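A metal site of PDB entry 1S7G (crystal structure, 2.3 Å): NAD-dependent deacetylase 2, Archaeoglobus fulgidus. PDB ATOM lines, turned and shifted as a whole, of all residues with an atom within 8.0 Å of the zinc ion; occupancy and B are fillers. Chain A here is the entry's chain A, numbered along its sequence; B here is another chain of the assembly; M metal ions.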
ATOM      1  N   LYS A  16      -8.927  -2.107   8.508  1.00  0.00           N
ATOM      2  CA  LYS A  16      -7.556  -1.902   8.068  1.00  0.00           C
ATOM      3  C   LYS A  16      -7.471  -1.509   6.595  1.00  0.00           C
ATOM      4  O   LYS A  16      -6.379  -1.316   6.066  1.00  0.00           O
ATOM      5  CB  LYS A  16      -6.734  -3.176   8.323  1.00  0.00           C
ATOM      6  N   HIS A  17      -8.616  -1.397   5.933  1.00  0.00           N
ATOM      7  CA  HIS A  17      -8.616  -1.029   4.520  1.00  0.00           C
ATOM      8  C   HIS A  17      -9.911  -0.338   4.151  1.00  0.00           C
ATOM      9  O   HIS A  17     -10.670  -0.823   3.310  1.00  0.00           O
ATOM     10  CB  HIS A  17      -8.426  -2.280   3.668  1.00  0.00           C
ATOM     11  CG  HIS A  17      -7.874  -1.995   2.311  1.00  0.00           C
ATOM     12  ND1 HIS A  17      -6.574  -2.309   1.959  1.00  0.00           N
ATOM     13  CD2 HIS A  17      -8.432  -1.405   1.221  1.00  0.00           C
ATOM     14  CE1 HIS A  17      -6.360  -1.933   0.713  1.00  0.00           C
ATOM     15  NE2 HIS A  17      -7.464  -1.374   0.247  1.00  0.00           N
ATOM     16  N   ALA A  18     -10.156   0.798   4.784  1.00  0.00           N
ATOM     17  CA  ALA A  18     -11.375   1.558   4.543  1.00  0.00           C
ATOM     18  C   ALA A  18     -11.247   2.553   3.396  1.00  0.00           C
ATOM     19  O   ALA A  18     -10.185   3.120   3.154  1.00  0.00           O
ATOM     20  CB  ALA A  18     -11.781   2.285   5.808  1.00  0.00           C
ATOM     21  N   VAL A  19     -12.355   2.756   2.679  1.00  0.00           N
ATOM     22  CA  VAL A  19     -12.391   3.692   1.567  1.00  0.00           C
ATOM     23  C   VAL A  19     -13.420   4.792   1.861  1.00  0.00           C
ATOM     24  O   VAL A  19     -14.448   4.540   2.477  1.00  0.00           O
ATOM     25  CB  VAL A  19     -12.767   2.967   0.244  1.00  0.00           C
ATOM     26  CG1 VAL A  19     -12.798   3.944  -0.900  1.00  0.00           C
ATOM     27  CG2 VAL A  19     -11.769   1.871  -0.043  1.00  0.00           C
ATOM     28  N   VAL A  94      -7.765   4.387   6.504  1.00  0.00           N
ATOM     29  CA  VAL A  94      -8.238   4.707   5.160  1.00  0.00           C
ATOM     30  C   VAL A  94      -7.112   4.467   4.152  1.00  0.00           C
ATOM     31  O   VAL A  94      -5.983   4.955   4.322  1.00  0.00           O
ATOM     32  CB  VAL A  94      -8.707   6.191   5.080  1.00  0.00           C
ATOM     33  CG1 VAL A  94      -8.924   6.585   3.632  1.00  0.00           C
ATOM     34  CG2 VAL A  94      -9.995   6.369   5.866  1.00  0.00           C
ATOM     35  N   LYS A  95      -7.424   3.718   3.097  1.00  0.00           N
ATOM     36  CA  LYS A  95      -6.460   3.380   2.064  1.00  0.00           C
ATOM     37  C   LYS A  95      -6.714   4.068   0.746  1.00  0.00           C
ATOM     38  O   LYS A  95      -5.867   4.063  -0.148  1.00  0.00           O
ATOM     39  CB  LYS A  95      -6.450   1.857   1.850  1.00  0.00           C
ATOM     40  CG  LYS A  95      -5.763   1.081   2.944  1.00  0.00           C
ATOM     41  CD  LYS A  95      -4.286   1.398   2.993  1.00  0.00           C
ATOM     42  CE  LYS A  95      -3.552   0.485   3.952  1.00  0.00           C
ATOM     43  NZ  LYS A  95      -4.033   0.628   5.355  1.00  0.00           N
ATOM     44  N   ALA A  96      -7.891   4.661   0.602  1.00  0.00           N
ATOM     45  CA  ALA A  96      -8.216   5.354  -0.631  1.00  0.00           C
ATOM     46  C   ALA A  96      -9.372   6.315  -0.474  1.00  0.00           C
ATOM     47  O   ALA A  96     -10.269   6.103   0.326  1.00  0.00           O
ATOM     48  CB  ALA A  96      -8.543   4.337  -1.714  1.00  0.00           C
ATOM     49  N   ARG A 113      -3.845   8.998  -1.748  1.00  0.00           N
ATOM     50  CA  ARG A 113      -4.547   8.248  -2.786  1.00  0.00           C
ATOM     51  C   ARG A 113      -5.949   8.775  -3.011  1.00  0.00           C
ATOM     52  O   ARG A 113      -6.853   8.521  -2.215  1.00  0.00           O
ATOM     53  CB  ARG A 113      -4.589   6.765  -2.442  1.00  0.00           C
ATOM     54  CG  ARG A 113      -5.231   5.902  -3.520  1.00  0.00           C
ATOM     55  CD  ARG A 113      -4.903   4.430  -3.284  1.00  0.00           C
ATOM     56  NE  ARG A 113      -5.558   3.526  -4.224  1.00  0.00           N
ATOM     57  CZ  ARG A 113      -5.384   3.549  -5.542  1.00  0.00           C
ATOM     58  NH1 ARG A 113      -6.030   2.677  -6.300  1.00  0.00           N
ATOM     59  NH2 ARG A 113      -4.582   4.453  -6.100  1.00  0.00           N
ATOM     60  N   LEU A 115      -8.886   9.058  -6.072  1.00  0.00           N
ATOM     61  CA  LEU A 115      -9.349   8.670  -7.397  1.00  0.00           C
ATOM     62  C   LEU A 115     -10.408   9.696  -7.786  1.00  0.00           C
ATOM     63  O   LEU A 115     -11.502   9.731  -7.219  1.00  0.00           O
ATOM     64  CB  LEU A 115      -9.929   7.244  -7.351  1.00  0.00           C
ATOM     65  CG  LEU A 115      -8.945   6.184  -6.845  1.00  0.00           C
ATOM     66  CD1 LEU A 115      -9.617   4.824  -6.766  1.00  0.00           C
ATOM     67  CD2 LEU A 115      -7.740   6.105  -7.793  1.00  0.00           C
ATOM     68  N   GLU A 176     -10.408   1.421 -11.072  1.00  0.00           N
ATOM     69  CA  GLU A 176      -9.721   1.334  -9.793  1.00  0.00           C
ATOM     70  C   GLU A 176     -10.688   1.606  -8.632  1.00  0.00           C
ATOM     71  O   GLU A 176     -10.604   0.972  -7.580  1.00  0.00           O
ATOM     72  CB  GLU A 176      -8.579   2.359  -9.731  1.00  0.00           C
ATOM     73  CG  GLU A 176      -7.200   1.815 -10.042  1.00  0.00           C
ATOM     74  CD  GLU A 176      -6.106   2.804  -9.679  1.00  0.00           C
ATOM     75  OE1 GLU A 176      -6.039   3.897 -10.283  1.00  0.00           O
ATOM     76  OE2 GLU A 176      -5.313   2.503  -8.755  1.00  0.00           O
ATOM     77  N   ALA A 177     -11.602   2.548  -8.815  1.00  0.00           N
ATOM     78  CA  ALA A 177     -12.569   2.878  -7.761  1.00  0.00           C
ATOM     79  C   ALA A 177     -13.444   1.662  -7.449  1.00  0.00           C
ATOM     80  O   ALA A 177     -13.687   1.353  -6.282  1.00  0.00           O
ATOM     81  CB  ALA A 177     -13.445   4.062  -8.189  1.00  0.00           C
ATOM     82  N   GLU A 179     -12.721  -1.556  -8.064  1.00  0.00           N
ATOM     83  CA  GLU A 179     -11.947  -2.611  -7.425  1.00  0.00           C
ATOM     84  C   GLU A 179     -11.839  -2.254  -5.944  1.00  0.00           C
ATOM     85  O   GLU A 179     -11.930  -3.112  -5.066  1.00  0.00           O
ATOM     86  CB  GLU A 179     -10.545  -2.711  -8.024  1.00  0.00           C
ATOM     87  CG  GLU A 179      -9.577  -3.547  -7.175  1.00  0.00           C
ATOM     88  CD  GLU A 179     -10.103  -4.941  -6.848  1.00  0.00           C
ATOM     89  OE1 GLU A 179      -9.554  -5.594  -5.928  1.00  0.00           O
ATOM     90  OE2 GLU A 179     -11.065  -5.408  -7.504  1.00  0.00           O
ATOM     91  N   GLU A 180     -11.677  -0.972  -5.674  1.00  0.00           N
ATOM     92  CA  GLU A 180     -11.560  -0.482  -4.321  1.00  0.00           C
ATOM     93  C   GLU A 180     -12.817  -0.805  -3.509  1.00  0.00           C
ATOM     94  O   GLU A 180     -12.740  -1.253  -2.374  1.00  0.00           O
ATOM     95  CB  GLU A 180     -11.319   1.040  -4.361  1.00  0.00           C
ATOM     96  CG  GLU A 180     -10.843   1.619  -3.080  1.00  0.00           C
ATOM     97  CD  GLU A 180      -9.641   0.873  -2.546  1.00  0.00           C
ATOM     98  OE1 GLU A 180      -9.791   0.198  -1.501  1.00  0.00           O
ATOM     99  OE2 GLU A 180      -8.557   0.946  -3.152  1.00  0.00           O
ATOM    100  N   ALA A 181     -13.992  -0.589  -4.097  1.00  0.00           N
ATOM    101  CA  ALA A 181     -15.237  -0.875  -3.394  1.00  0.00           C
ATOM    102  C   ALA A 181     -15.416  -2.367  -3.152  1.00  0.00           C
ATOM    103  O   ALA A 181     -16.057  -2.758  -2.176  1.00  0.00           O
ATOM    104  CB  ALA A 181     -16.432  -0.327  -4.183  1.00  0.00           C
ATOM    105  N   LYS A 182     -14.846  -3.197  -4.021  1.00  0.00           N
ATOM    106  CA  LYS A 182     -14.980  -4.649  -3.902  1.00  0.00           C
ATOM    107  C   LYS A 182     -14.082  -5.329  -2.874  1.00  0.00           C
ATOM    108  O   LYS A 182     -14.387  -6.435  -2.437  1.00  0.00           O
ATOM    109  CB  LYS A 182     -14.759  -5.319  -5.262  1.00  0.00           C
ATOM    110  CG  LYS A 182     -15.939  -5.192  -6.208  1.00  0.00           C
ATOM    111  CD  LYS A 182     -15.736  -6.068  -7.448  1.00  0.00           C
ATOM    112  CE  LYS A 182     -16.932  -5.980  -8.398  1.00  0.00           C
ATOM    113  NZ  LYS A 182     -16.700  -6.760  -9.642  1.00  0.00           N
ATOM    114  N   HIS A 183     -12.981  -4.691  -2.497  1.00  0.00           N
ATOM    115  CA  HIS A 183     -12.102  -5.333  -1.530  1.00  0.00           C
ATOM    116  C   HIS A 183     -11.885  -4.546  -0.238  1.00  0.00           C
ATOM    117  O   HIS A 183     -11.078  -4.935   0.592  1.00  0.00           O
ATOM    118  CB  HIS A 183     -10.751  -5.682  -2.183  1.00  0.00           C
ATOM    119  CG  HIS A 183      -9.869  -4.506  -2.443  1.00  0.00           C
ATOM    120  ND1 HIS A 183      -9.240  -4.307  -3.659  1.00  0.00           N
ATOM    121  CD2 HIS A 183      -9.474  -3.486  -1.643  1.00  0.00           C
ATOM    122  CE1 HIS A 183      -8.486  -3.229  -3.582  1.00  0.00           C
ATOM    123  NE2 HIS A 183      -8.610  -2.706  -2.378  1.00  0.00           N
ATOM    124  N   CYS A 184     -12.601  -3.440  -0.068  1.00  0.00           N
ATOM    125  CA  CYS A 184     -12.447  -2.667   1.166  1.00  0.00           C
ATOM    126  C   CYS A 184     -13.211  -3.393   2.291  1.00  0.00           C
ATOM    127  O   CYS A 184     -14.082  -4.215   2.011  1.00  0.00           O
ATOM    128  CB  CYS A 184     -13.011  -1.249   1.000  1.00  0.00           C
ATOM    129  SG  CYS A 184     -14.830  -1.126   0.779  1.00  0.00           S
ATOM    130  N   ASP A 185     -12.879  -3.105   3.540  1.00  0.00           N
ATOM    131  CA  ASP A 185     -13.581  -3.731   4.647  1.00  0.00           C
ATOM    132  C   ASP A 185     -14.532  -2.733   5.301  1.00  0.00           C
ATOM    133  O   ASP A 185     -15.380  -3.088   6.101  1.00  0.00           O
ATOM    134  CB  ASP A 185     -12.589  -4.341   5.655  1.00  0.00           C
ATOM    135  CG  ASP A 185     -11.645  -3.315   6.262  1.00  0.00           C
ATOM    136  OD1 ASP A 185     -11.310  -2.327   5.593  1.00  0.00           O
ATOM    137  OD2 ASP A 185     -11.229  -3.522   7.425  1.00  0.00           O
ATOM    138  N   CYS B 126       1.289  -1.222  -6.229  1.00  0.00           N
ATOM    139  CA  CYS B 126       1.045  -2.441  -5.483  1.00  0.00           C
ATOM    140  C   CYS B 126      -0.472  -2.549  -5.440  1.00  0.00           C
ATOM    141  O   CYS B 126      -1.140  -1.607  -5.009  1.00  0.00           O
ATOM    142  CB  CYS B 126       1.582  -2.350  -4.053  1.00  0.00           C
ATOM    143  SG  CYS B 126       1.159  -3.835  -3.073  1.00  0.00           S
ATOM    144  N   LEU B 127      -1.010  -3.679  -5.876  1.00  0.00           N
ATOM    145  CA  LEU B 127      -2.452  -3.890  -5.885  1.00  0.00           C
ATOM    146  C   LEU B 127      -3.035  -4.172  -4.506  1.00  0.00           C
ATOM    147  O   LEU B 127      -4.246  -4.102  -4.314  1.00  0.00           O
ATOM    148  CB  LEU B 127      -2.793  -5.057  -6.813  1.00  0.00           C
ATOM    149  CG  LEU B 127      -2.393  -4.920  -8.280  1.00  0.00           C
ATOM    150  CD1 LEU B 127      -2.833  -6.156  -9.045  1.00  0.00           C
ATOM    151  CD2 LEU B 127      -3.033  -3.679  -8.870  1.00  0.00           C
ATOM    152  N   ASP B 128      -2.177  -4.475  -3.540  1.00  0.00           N
ATOM    153  CA  ASP B 128      -2.659  -4.772  -2.197  1.00  0.00           C
ATOM    154  C   ASP B 128      -2.700  -3.560  -1.276  1.00  0.00           C
ATOM    155  O   ASP B 128      -3.736  -3.308  -0.657  1.00  0.00           O
ATOM    156  CB  ASP B 128      -1.806  -5.869  -1.554  1.00  0.00           C
ATOM    157  CG  ASP B 128      -2.079  -7.238  -2.160  1.00  0.00           C
ATOM    158  OD1 ASP B 128      -3.256  -7.671  -2.147  1.00  0.00           O
ATOM    159  OD2 ASP B 128      -1.119  -7.889  -2.636  1.00  0.00           O
ATOM    160  N   CYS B 129      -1.603  -2.804  -1.192  1.00  0.00           N
ATOM    161  CA  CYS B 129      -1.560  -1.645  -0.312  1.00  0.00           C
ATOM    162  C   CYS B 129      -1.535  -0.304  -1.061  1.00  0.00           C
ATOM    163  O   CYS B 129      -1.550   0.760  -0.440  1.00  0.00           O
ATOM    164  CB  CYS B 129      -0.349  -1.721   0.611  1.00  0.00           C
ATOM    165  SG  CYS B 129       1.154  -1.098  -0.146  1.00  0.00           S
ATOM    166  N   HIS B 130      -1.478  -0.378  -2.384  1.00  0.00           N
ATOM    167  CA  HIS B 130      -1.471   0.799  -3.250  1.00  0.00           C
ATOM    168  C   HIS B 130      -0.230   1.676  -3.267  1.00  0.00           C
ATOM    169  O   HIS B 130      -0.291   2.813  -3.719  1.00  0.00           O
ATOM    170  CB  HIS B 130      -2.697   1.660  -2.969  1.00  0.00           C
ATOM    171  CG  HIS B 130      -3.981   0.897  -3.048  1.00  0.00           C
ATOM    172  ND1 HIS B 130      -4.346   0.209  -4.183  1.00  0.00           N
ATOM    173  CD2 HIS B 130      -4.926   0.638  -2.119  1.00  0.00           C
ATOM    174  CE1 HIS B 130      -5.467  -0.448  -3.943  1.00  0.00           C
ATOM    175  NE2 HIS B 130      -5.836  -0.204  -2.707  1.00  0.00           N
HETATM  176 ZN    ZN M   1      -7.650  -0.807  -1.780  1.00  0.00          ZN
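O of Glu 180 sits close to SG of Cys 184 (3.8 Å).
The backbone NH (N) of His 17 sits close to the side-chain carboxylate (OD1) of Asp 185 (2.9 Å).
The side-chain carboxylate (OE1) of Glu 179 sits at hydrogen-bond distance from a ring nitrogen (ND1) of His 183, 2.6 Å away.
Within 4 Å of the zinc ion: His 17, Glu 180, His 183 and His 130 of chain B.
A ring nitrogen (NE2) of His 17 binds the zinc ion (2.1 Å).
A ring nitrogen (NE2) of His 130 of chain B binds the zinc ion (2.1 Å).
NE2 of His 183 is bound to the zinc ion.
OE1 of Glu 180 is bound to the zinc ion (2.4 Å).
The zinc ion is bound by OE2 of Glu 180, 2.4 Å away.
The zinc ion has five donor atoms within binding distance.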
